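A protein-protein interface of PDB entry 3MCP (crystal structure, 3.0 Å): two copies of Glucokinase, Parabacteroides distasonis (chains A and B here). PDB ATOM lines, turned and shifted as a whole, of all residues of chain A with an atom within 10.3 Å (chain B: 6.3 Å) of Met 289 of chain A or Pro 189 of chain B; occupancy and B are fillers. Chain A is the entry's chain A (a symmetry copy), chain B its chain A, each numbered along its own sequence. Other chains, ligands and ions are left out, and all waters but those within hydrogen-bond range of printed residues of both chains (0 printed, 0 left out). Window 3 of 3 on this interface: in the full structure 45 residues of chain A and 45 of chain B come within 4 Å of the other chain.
The backbone NH (N) of Asn 185 of chain B is in hydrogen-bond range of the backbone carbonyl oxygen (O) of Tyr 191 of chain B (3.1 Å). The side-chain amide nitrogen of Asn 185 of chain B is in hydrogen-bond range of the backbone carbonyl oxygen of Ile 192 of chain B (3.1 Å). The backbone carbonyl oxygen of Asp 249 of chain A lies within hydrogen-bond range of the side-chain hydroxyl of Ser 253 of chain A (3.2 Å). OD1 of Asp 249 of chain A sits close to OE1 of Gln 286 of chain A, 2.9 Å away. The side-chain hydroxyl (OG1) of Thr 256 of chain A lies within hydrogen-bond range of the backbone carbonyl oxygen (O) of Ala 252 of chain A (3.0 Å).
Among the printed residues, merely in contact across the chains: Asp 249 of chain A with Arg 184 of chain B (3.97 Å), Ser 253 of chain A with Leu 183 of chain B (3.4 Å), Thr 256 of chain A with Cys 182 of chain B (3.7 Å), Met 289 of chain A with Pro 189 of chain B (3.6 Å), Met 289 of chain A with Tyr 191 of chain B (3.9 Å), Met 289 of chain A with Ile 192 of chain B (3.9 Å) and Met 290 of chain A with Cys 182 of chain B (3.6 Å).
Of the printed residues of chain B, Asp 249 of chain A touches Arg 184. Of the printed residues of chain B, Thr 256 of chain A touches Cys 182. Printed residues of chain B within 4 Å of Met 289 of chain A: Pro 189 (3.6 Å), Tyr 191 (3.9 Å) and Ile 192 (3.9 Å). Printed residues of chain B within 4 Å of Met 290 of chain A: Cys 182 (3.6 Å). Printed residues of chain A within 4 Å of Arg 184 of chain B: Asp 249. Pro 189 of chain B touches one residue of chain A. The nearest residue of chain A that does not touch Pro 189 of chain B is Lys 186 of chain A (7.1 Å). The nearest printed residue of chain B that does not touch Met 290 of chain A is Ile 192 of chain B (4.9 Å).
Of the 11 printed residues of chain B, 6 touch a printed residue of chain A. Hydrophobic or aromatic side chains of chain B within 4 Å of the printed part of chain A: Leu 183 and Ile 192. Of the 22 printed residues of chain A, 5 touch a printed residue of chain B. Hydrophobic or aromatic side chains of chain A that line the printed part of chain B: Met 289 and Met 290. Along chain A the printed residues that touch a printed residue of chain B span positions 249 to 290.
Positions printed for both chains: 184, 185, 186, 187 and 189.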
ATOM      1  N   ARG A 184       9.788 -14.045  32.524  1.00  0.00           N
ATOM      2  CA  ARG A 184      11.139 -13.503  32.339  1.00  0.00           C
ATOM      3  C   ARG A 184      11.198 -12.646  31.065  1.00  0.00           C
ATOM      4  O   ARG A 184      10.618 -12.999  30.048  1.00  0.00           O
ATOM      5  CB  ARG A 184      12.176 -14.642  32.287  1.00  0.00           C
ATOM      6  CG  ARG A 184      13.641 -14.193  32.473  1.00  0.00           C
ATOM      7  CD  ARG A 184      14.619 -15.391  32.499  1.00  0.00           C
ATOM      8  N   ASN A 185      11.859 -11.494  31.159  1.00  0.00           N
ATOM      9  CA  ASN A 185      12.009 -10.571  30.032  1.00  0.00           C
ATOM     10  C   ASN A 185      13.108 -11.070  29.105  1.00  0.00           C
ATOM     11  O   ASN A 185      14.186 -11.430  29.559  1.00  0.00           O
ATOM     12  CB  ASN A 185      12.350  -9.177  30.561  1.00  0.00           C
ATOM     13  CG  ASN A 185      12.251  -8.106  29.507  1.00  0.00           C
ATOM     14  OD1 ASN A 185      12.867  -8.200  28.445  1.00  0.00           O
ATOM     15  ND2 ASN A 185      11.508  -7.043  29.815  1.00  0.00           N
ATOM     16  N   LYS A 186      12.831 -11.092  27.806  1.00  0.00           N
ATOM     17  CA  LYS A 186      13.775 -11.638  26.816  1.00  0.00           C
ATOM     18  C   LYS A 186      15.076 -10.817  26.706  1.00  0.00           C
ATOM     19  O   LYS A 186      16.172 -11.370  26.794  1.00  0.00           O
ATOM     20  CB  LYS A 186      13.099 -11.719  25.450  1.00  0.00           C
ATOM     21  CG  LYS A 186      13.936 -12.374  24.356  1.00  0.00           C
ATOM     22  CD  LYS A 186      13.356 -12.068  22.958  1.00  0.00           C
ATOM     23  CE  LYS A 186      14.322 -12.448  21.830  1.00  0.00           C
ATOM     24  NZ  LYS A 186      13.897 -11.845  20.546  1.00  0.00           N
ATOM     25  N   LYS A 187      14.941  -9.503  26.501  1.00  0.00           N
ATOM     26  CA  LYS A 187      16.105  -8.609  26.338  1.00  0.00           C
ATOM     27  C   LYS A 187      16.619  -8.013  27.655  1.00  0.00           C
ATOM     28  O   LYS A 187      17.512  -7.166  27.644  1.00  0.00           O
ATOM     29  CB  LYS A 187      15.774  -7.454  25.373  1.00  0.00           C
ATOM     30  CG  LYS A 187      15.872  -7.794  23.879  1.00  0.00           C
ATOM     31  CD  LYS A 187      16.059  -6.495  23.041  1.00  0.00           C
ATOM     32  CE  LYS A 187      15.976  -6.741  21.526  1.00  0.00           C
ATOM     33  NZ  LYS A 187      16.115  -5.458  20.753  1.00  0.00           N
ATOM     34  N   PRO A 189      16.964 -10.153  30.959  1.00  0.00           N
ATOM     35  CA  PRO A 189      16.842 -11.377  31.783  1.00  0.00           C
ATOM     36  C   PRO A 189      16.655 -11.165  33.298  1.00  0.00           C
ATOM     37  O   PRO A 189      16.014 -11.991  33.960  1.00  0.00           O
ATOM     38  CB  PRO A 189      18.156 -12.102  31.518  1.00  0.00           C
ATOM     39  CG  PRO A 189      18.554 -11.672  30.161  1.00  0.00           C
ATOM     40  CD  PRO A 189      18.064 -10.266  29.983  1.00  0.00           C
ATOM     41  N   ASP A 249       7.353 -12.820  22.681  1.00  0.00           N
ATOM     42  CA  ASP A 249       8.122 -13.850  23.387  1.00  0.00           C
ATOM     43  C   ASP A 249       7.317 -14.417  24.564  1.00  0.00           C
ATOM     44  O   ASP A 249       7.259 -15.629  24.764  1.00  0.00           O
ATOM     45  CB  ASP A 249       9.465 -13.274  23.883  1.00  0.00           C
ATOM     46  CG  ASP A 249      10.277 -14.285  24.701  1.00  0.00           C
ATOM     47  OD1 ASP A 249      10.752 -15.297  24.126  1.00  0.00           O
ATOM     48  OD2 ASP A 249      10.462 -14.045  25.919  1.00  0.00           O
ATOM     49  N   ALA A 252       4.228 -16.256  23.263  1.00  0.00           N
ATOM     50  CA  ALA A 252       4.684 -17.521  22.680  1.00  0.00           C
ATOM     51  C   ALA A 252       4.778 -18.617  23.726  1.00  0.00           C
ATOM     52  O   ALA A 252       4.155 -19.665  23.590  1.00  0.00           O
ATOM     53  CB  ALA A 252       6.015 -17.338  22.015  1.00  0.00           C
ATOM     54  N   SER A 253       5.549 -18.373  24.779  1.00  0.00           N
ATOM     55  CA  SER A 253       5.759 -19.391  25.816  1.00  0.00           C
ATOM     56  C   SER A 253       4.516 -19.615  26.685  1.00  0.00           C
ATOM     57  O   SER A 253       4.326 -20.696  27.228  1.00  0.00           O
ATOM     58  CB  SER A 253       6.999 -19.062  26.678  1.00  0.00           C
ATOM     59  OG  SER A 253       6.997 -17.723  27.111  1.00  0.00           O
ATOM     60  N   THR A 256       2.033 -21.770  24.500  1.00  0.00           N
ATOM     61  CA  THR A 256       2.526 -23.139  24.351  1.00  0.00           C
ATOM     62  C   THR A 256       1.840 -24.086  25.332  1.00  0.00           C
ATOM     63  O   THR A 256       1.565 -25.232  24.994  1.00  0.00           O
ATOM     64  CB  THR A 256       4.036 -23.227  24.561  1.00  0.00           C
ATOM     65  OG1 THR A 256       4.709 -22.561  23.480  1.00  0.00           O
ATOM     66  CG2 THR A 256       4.485 -24.684  24.617  1.00  0.00           C
ATOM     67  N   LYS A 281       5.982 -11.910  14.262  1.00  0.00           N
ATOM     68  CA  LYS A 281       7.279 -12.369  13.770  1.00  0.00           C
ATOM     69  C   LYS A 281       7.999 -13.192  14.865  1.00  0.00           C
ATOM     70  O   LYS A 281       8.583 -14.251  14.581  1.00  0.00           O
ATOM     71  CB  LYS A 281       8.142 -11.169  13.317  1.00  0.00           C
ATOM     72  CG  LYS A 281       9.488 -11.547  12.647  1.00  0.00           C
ATOM     73  CD  LYS A 281      10.310 -10.287  12.260  1.00  0.00           C
ATOM     74  CE  LYS A 281      11.659 -10.650  11.614  1.00  0.00           C
ATOM     75  N   GLU A 282       7.908 -12.719  16.114  1.00  0.00           N
ATOM     76  CA  GLU A 282       8.553 -13.384  17.255  1.00  0.00           C
ATOM     77  C   GLU A 282       7.909 -14.692  17.636  1.00  0.00           C
ATOM     78  O   GLU A 282       8.593 -15.637  18.046  1.00  0.00           O
ATOM     79  CB  GLU A 282       8.559 -12.470  18.482  1.00  0.00           C
ATOM     80  CG  GLU A 282       9.871 -11.756  18.697  1.00  0.00           C
ATOM     81  CD  GLU A 282      10.994 -12.700  19.130  1.00  0.00           C
ATOM     82  OE1 GLU A 282      10.796 -13.466  20.109  1.00  0.00           O
ATOM     83  OE2 GLU A 282      12.077 -12.657  18.503  1.00  0.00           O
ATOM     84  N   MET A 283       6.588 -14.739  17.567  1.00  0.00           N
ATOM     85  CA  MET A 283       5.870 -15.930  17.941  1.00  0.00           C
ATOM     86  C   MET A 283       6.190 -17.046  16.969  1.00  0.00           C
ATOM     87  O   MET A 283       6.357 -18.196  17.384  1.00  0.00           O
ATOM     88  CB  MET A 283       4.362 -15.664  18.013  1.00  0.00           C
ATOM     89  CG  MET A 283       3.978 -14.697  19.131  1.00  0.00           C
ATOM     90  SD  MET A 283       2.088 -14.636  19.510  1.00  0.00           S
ATOM     91  CE  MET A 283       1.876 -16.419  20.206  1.00  0.00           C
ATOM     92  N   ASN A 284       6.358 -16.696  15.689  1.00  0.00           N
ATOM     93  CA  ASN A 284       6.644 -17.692  14.640  1.00  0.00           C
ATOM     94  C   ASN A 284       8.108 -18.080  14.541  1.00  0.00           C
ATOM     95  O   ASN A 284       8.448 -19.074  13.903  1.00  0.00           O
ATOM     96  CB  ASN A 284       6.142 -17.200  13.292  1.00  0.00           C
ATOM     97  CG  ASN A 284       4.643 -17.147  13.225  1.00  0.00           C
ATOM     98  OD1 ASN A 284       3.969 -18.159  13.401  1.00  0.00           O
ATOM     99  ND2 ASN A 284       4.106 -15.966  12.973  1.00  0.00           N
ATOM    100  N   ALA A 285       8.976 -17.288  15.155  1.00  0.00           N
ATOM    101  CA  ALA A 285      10.388 -17.629  15.220  1.00  0.00           C
ATOM    102  C   ALA A 285      10.601 -18.659  16.333  1.00  0.00           C
ATOM    103  O   ALA A 285      11.404 -19.592  16.185  1.00  0.00           O
ATOM    104  CB  ALA A 285      11.215 -16.394  15.474  1.00  0.00           C
ATOM    105  N   GLN A 286       9.826 -18.504  17.422  1.00  0.00           N
ATOM    106  CA  GLN A 286       9.945 -19.353  18.635  1.00  0.00           C
ATOM    107  C   GLN A 286       9.274 -20.738  18.503  1.00  0.00           C
ATOM    108  O   GLN A 286       9.866 -21.757  18.860  1.00  0.00           O
ATOM    109  CB  GLN A 286       9.392 -18.609  19.862  1.00  0.00           C
ATOM    110  CG  GLN A 286       9.484 -19.418  21.167  1.00  0.00           C
ATOM    111  CD  GLN A 286       9.440 -18.547  22.417  1.00  0.00           C
ATOM    112  OE1 GLN A 286       9.733 -17.349  22.362  1.00  0.00           O
ATOM    113  NE2 GLN A 286       9.107 -19.160  23.562  1.00  0.00           N
ATOM    114  N   THR A 287       8.039 -20.772  18.011  1.00  0.00           N
ATOM    115  CA  THR A 287       7.373 -22.054  17.750  1.00  0.00           C
ATOM    116  C   THR A 287       7.895 -22.663  16.422  1.00  0.00           C
ATOM    117  O   THR A 287       7.381 -23.684  15.954  1.00  0.00           O
ATOM    118  CB  THR A 287       5.821 -21.912  17.705  1.00  0.00           C
ATOM    119  OG1 THR A 287       5.450 -20.987  16.675  1.00  0.00           O
ATOM    120  CG2 THR A 287       5.264 -21.426  19.069  1.00  0.00           C
ATOM    121  N   GLY A 288       8.908 -22.015  15.828  1.00  0.00           N
ATOM    122  CA  GLY A 288       9.551 -22.494  14.600  1.00  0.00           C
ATOM    123  C   GLY A 288      10.740 -23.391  14.896  1.00  0.00           C
ATOM    124  O   GLY A 288      11.126 -24.220  14.066  1.00  0.00           O
ATOM    125  N   MET A 289      11.345 -23.208  16.075  1.00  0.00           N
ATOM    126  CA  MET A 289      12.448 -24.070  16.528  1.00  0.00           C
ATOM    127  C   MET A 289      11.978 -25.542  16.441  1.00  0.00           C
ATOM    128  O   MET A 289      12.689 -26.408  15.910  1.00  0.00           O
ATOM    129  CB  MET A 289      12.868 -23.718  17.972  1.00  0.00           C
ATOM    130  CG  MET A 289      13.370 -22.261  18.168  1.00  0.00           C
ATOM    131  SD  MET A 289      13.676 -21.775  20.072  1.00  0.00           S
ATOM    132  CE  MET A 289      13.988 -19.847  19.867  1.00  0.00           C
ATOM    133  N   MET A 290      10.758 -25.793  16.939  1.00  0.00           N
ATOM    134  CA  MET A 290      10.122 -27.126  16.892  1.00  0.00           C
ATOM    135  C   MET A 290      10.572 -27.917  15.647  1.00  0.00           C
ATOM    136  O   MET A 290      10.478 -29.149  15.602  1.00  0.00           O
ATOM    137  CB  MET A 290       8.577 -26.988  16.885  1.00  0.00           C
ATOM    138  CG  MET A 290       7.969 -26.199  18.091  1.00  0.00           C
ATOM    139  SD  MET A 290       5.985 -26.002  18.013  1.00  0.00           S
ATOM    140  CE  MET A 290       5.728 -24.756  19.501  1.00  0.00           C
ATOM    141  N   GLN A 299       6.005 -26.772  13.459  1.00  0.00           N
ATOM    142  CA  GLN A 299       4.788 -27.525  13.750  1.00  0.00           C
ATOM    143  C   GLN A 299       3.681 -26.654  14.353  1.00  0.00           C
ATOM    144  O   GLN A 299       2.748 -27.176  14.969  1.00  0.00           O
ATOM    145  CB  GLN A 299       5.091 -28.675  14.719  1.00  0.00           C
ATOM    146  CG  GLN A 299       5.614 -29.930  14.067  1.00  0.00           C
ATOM    147  CD  GLN A 299       5.405 -31.152  14.944  1.00  0.00           C
ATOM    148  OE1 GLN A 299       5.421 -31.059  16.174  1.00  0.00           O
ATOM    149  NE2 GLN A 299       5.184 -32.300  14.315  1.00  0.00           N
ATOM    150  N   LYS A 300       3.769 -25.341  14.177  1.00  0.00           N
ATOM    151  CA  LYS A 300       2.786 -24.446  14.766  1.00  0.00           C
ATOM    152  C   LYS A 300       2.931 -23.066  14.172  1.00  0.00           C
ATOM    153  O   LYS A 300       3.989 -22.462  14.275  1.00  0.00           O
ATOM    154  CB  LYS A 300       3.017 -24.363  16.269  1.00  0.00           C
ATOM    155  CG  LYS A 300       1.847 -23.815  17.078  1.00  0.00           C
ATOM    156  CD  LYS A 300       1.094 -24.929  17.796  1.00  0.00           C
ATOM    157  CE  LYS A 300       0.416 -24.410  19.065  1.00  0.00           C
ATOM    158  NZ  LYS A 300       0.028 -25.524  19.993  1.00  0.00           N
ATOM    159  N   GLU A 301       1.879 -22.564  13.538  1.00  0.00           N
ATOM    160  CA  GLU A 301       1.923 -21.225  12.983  1.00  0.00           C
ATOM    161  C   GLU A 301       0.918 -20.307  13.673  1.00  0.00           C
ATOM    162  O   GLU A 301      -0.155 -20.742  14.092  1.00  0.00           O
ATOM    163  CB  GLU A 301       1.684 -21.236  11.466  1.00  0.00           C
ATOM    164  CG  GLU A 301       1.966 -19.850  10.809  1.00  0.00           C
ATOM    165  CD  GLU A 301       1.898 -19.854   9.281  1.00  0.00           C
ATOM    166  OE1 GLU A 301       1.779 -20.941   8.681  1.00  0.00           O
ATOM    167  OE2 GLU A 301       1.976 -18.755   8.686  1.00  0.00           O
ATOM    168  N   CYS B 182       9.246 -27.420  24.253  1.00  0.00           N
ATOM    169  CA  CYS B 182       9.677 -26.486  23.228  1.00  0.00           C
ATOM    170  C   CYS B 182       9.769 -25.048  23.717  1.00  0.00           C
ATOM    171  O   CYS B 182       9.855 -24.128  22.912  1.00  0.00           O
ATOM    172  CB  CYS B 182       8.738 -26.562  22.041  1.00  0.00           C
ATOM    173  SG  CYS B 182       7.053 -26.281  22.478  1.00  0.00           S
ATOM    174  N   LEU B 183       9.742 -24.844  25.030  1.00  0.00           N
ATOM    175  CA  LEU B 183       9.923 -23.498  25.574  1.00  0.00           C
ATOM    176  C   LEU B 183      11.360 -23.077  25.306  1.00  0.00           C
ATOM    177  O   LEU B 183      12.225 -23.929  25.030  1.00  0.00           O
ATOM    178  CB  LEU B 183       9.627 -23.459  27.079  1.00  0.00           C
ATOM    179  CG  LEU B 183       8.164 -23.626  27.519  1.00  0.00           C
ATOM    180  CD1 LEU B 183       8.069 -23.809  29.019  1.00  0.00           C
ATOM    181  CD2 LEU B 183       7.352 -22.452  27.089  1.00  0.00           C
ATOM    182  N   ARG B 184      11.619 -21.774  25.375  1.00  0.00           N
ATOM    183  CA  ARG B 184      12.958 -21.246  25.092  1.00  0.00           C
ATOM    184  C   ARG B 184      13.944 -21.688  26.184  1.00  0.00           C
ATOM    185  O   ARG B 184      13.610 -21.699  27.360  1.00  0.00           O
ATOM    186  CB  ARG B 184      12.919 -19.710  24.970  1.00  0.00           C
ATOM    187  CG  ARG B 184      14.166 -19.081  24.313  1.00  0.00           C
ATOM    188  CD  ARG B 184      14.026 -17.550  24.142  1.00  0.00           C
ATOM    189  N   ASN B 185      15.139 -22.101  25.768  1.00  0.00           N
ATOM    190  CA  ASN B 185      16.190 -22.548  26.686  1.00  0.00           C
ATOM    191  C   ASN B 185      16.877 -21.338  27.303  1.00  0.00           C
ATOM    192  O   ASN B 185      17.240 -20.406  26.598  1.00  0.00           O
ATOM    193  CB  ASN B 185      17.200 -23.404  25.922  1.00  0.00           C
ATOM    194  CG  ASN B 185      18.158 -24.135  26.827  1.00  0.00           C
ATOM    195  OD1 ASN B 185      18.826 -23.529  27.666  1.00  0.00           O
ATOM    196  ND2 ASN B 185      18.272 -25.447  26.628  1.00  0.00           N
ATOM    197  N   LYS B 186      17.053 -21.356  28.620  1.00  0.00           N
ATOM    198  CA  LYS B 186      17.623 -20.209  29.347  1.00  0.00           C
ATOM    199  C   LYS B 186      19.093 -19.928  28.975  1.00  0.00           C
ATOM    200  O   LYS B 186      19.445 -18.799  28.635  1.00  0.00           O
ATOM    201  CB  LYS B 186      17.506 -20.443  30.851  1.00  0.00           C
ATOM    202  CG  LYS B 186      17.959 -19.275  31.720  1.00  0.00           C
ATOM    203  CD  LYS B 186      18.177 -19.725  33.181  1.00  0.00           C
ATOM    204  CE  LYS B 186      18.912 -18.669  34.013  1.00  0.00           C
ATOM    205  NZ  LYS B 186      19.400 -19.246  35.286  1.00  0.00           N
ATOM    206  N   LYS B 187      19.939 -20.959  29.056  1.00  0.00           N
ATOM    207  CA  LYS B 187      21.381 -20.817  28.767  1.00  0.00           C
ATOM    208  C   LYS B 187      21.746 -21.064  27.297  1.00  0.00           C
ATOM    209  O   LYS B 187      22.926 -21.086  26.947  1.00  0.00           O
ATOM    210  CB  LYS B 187      22.210 -21.774  29.645  1.00  0.00           C
ATOM    211  CG  LYS B 187      22.486 -21.285  31.075  1.00  0.00           C
ATOM    212  CD  LYS B 187      23.728 -22.016  31.664  1.00  0.00           C
ATOM    213  CE  LYS B 187      23.950 -21.716  33.155  1.00  0.00           C
ATOM    214  NZ  LYS B 187      25.129 -22.474  33.698  1.00  0.00           N
ATOM    215  N   TYR B 188      20.744 -21.282  26.452  1.00  0.00           N
ATOM    216  CA  TYR B 188      20.980 -21.528  25.026  1.00  0.00           C
ATOM    217  C   TYR B 188      19.824 -20.965  24.201  1.00  0.00           C
ATOM    218  O   TYR B 188      19.188 -21.693  23.456  1.00  0.00           O
ATOM    219  CB  TYR B 188      21.130 -23.033  24.764  1.00  0.00           C
ATOM    220  CG  TYR B 188      22.278 -23.693  25.516  1.00  0.00           C
ATOM    221  CD1 TYR B 188      23.590 -23.590  25.057  1.00  0.00           C
ATOM    222  CD2 TYR B 188      22.047 -24.434  26.664  1.00  0.00           C
ATOM    223  CE1 TYR B 188      24.647 -24.204  25.733  1.00  0.00           C
ATOM    224  CE2 TYR B 188      23.098 -25.051  27.350  1.00  0.00           C
ATOM    225  CZ  TYR B 188      24.392 -24.930  26.877  1.00  0.00           C
ATOM    226  OH  TYR B 188      25.429 -25.537  27.546  1.00  0.00           O
ATOM    227  N   PRO B 189      19.583 -19.646  24.308  1.00  0.00           N
ATOM    228  CA  PRO B 189      18.439 -18.926  23.705  1.00  0.00           C
ATOM    229  C   PRO B 189      18.010 -19.383  22.296  1.00  0.00           C
ATOM    230  O   PRO B 189      16.827 -19.282  21.952  1.00  0.00           O
ATOM    231  CB  PRO B 189      18.930 -17.484  23.656  1.00  0.00           C
ATOM    232  CG  PRO B 189      19.886 -17.375  24.778  1.00  0.00           C
ATOM    233  CD  PRO B 189      20.544 -18.714  24.927  1.00  0.00           C
ATOM    234  N   GLU B 190      18.962 -19.854  21.493  1.00  0.00           N
ATOM    235  CA  GLU B 190      18.664 -20.296  20.134  1.00  0.00           C
ATOM    236  C   GLU B 190      18.045 -21.719  20.084  1.00  0.00           C
ATOM    237  O   GLU B 190      17.528 -22.131  19.051  1.00  0.00           O
ATOM    238  CB  GLU B 190      19.933 -20.231  19.274  1.00  0.00           C
ATOM    239  N   TYR B 191      18.078 -22.442  21.206  1.00  0.00           N
ATOM    240  CA  TYR B 191      17.524 -23.818  21.276  1.00  0.00           C
ATOM    241  C   TYR B 191      16.336 -23.956  22.265  1.00  0.00           C
ATOM    242  O   TYR B 191      16.007 -23.024  22.992  1.00  0.00           O
ATOM    243  CB  TYR B 191      18.615 -24.801  21.672  1.00  0.00           C
ATOM    244  CG  TYR B 191      19.776 -24.857  20.712  1.00  0.00           C
ATOM    245  CD1 TYR B 191      20.843 -23.966  20.826  1.00  0.00           C
ATOM    246  CD2 TYR B 191      19.830 -25.830  19.710  1.00  0.00           C
ATOM    247  CE1 TYR B 191      21.923 -24.025  19.962  1.00  0.00           C
ATOM    248  CE2 TYR B 191      20.910 -25.902  18.837  1.00  0.00           C
ATOM    249  CZ  TYR B 191      21.954 -24.995  18.966  1.00  0.00           C
ATOM    250  OH  TYR B 191      23.027 -25.054  18.105  1.00  0.00           O
ATOM    251  N   ILE B 192      15.709 -25.132  22.269  1.00  0.00           N
ATOM    252  CA  ILE B 192      14.586 -25.416  23.167  1.00  0.00           C
ATOM    253  C   ILE B 192      15.091 -26.018  24.468  1.00  0.00           C
ATOM    254  O   ILE B 192      16.222 -26.499  24.530  1.00  0.00           O
ATOM    255  CB  ILE B 192      13.593 -26.384  22.526  1.00  0.00           C
ATOM    256  CG1 ILE B 192      14.253 -27.746  22.248  1.00  0.00           C
ATOM    257  CG2 ILE B 192      13.048 -25.793  21.251  1.00  0.00           C
ATOM    258  CD1 ILE B 192      13.306 -28.770  21.666  1.00  0.00           C
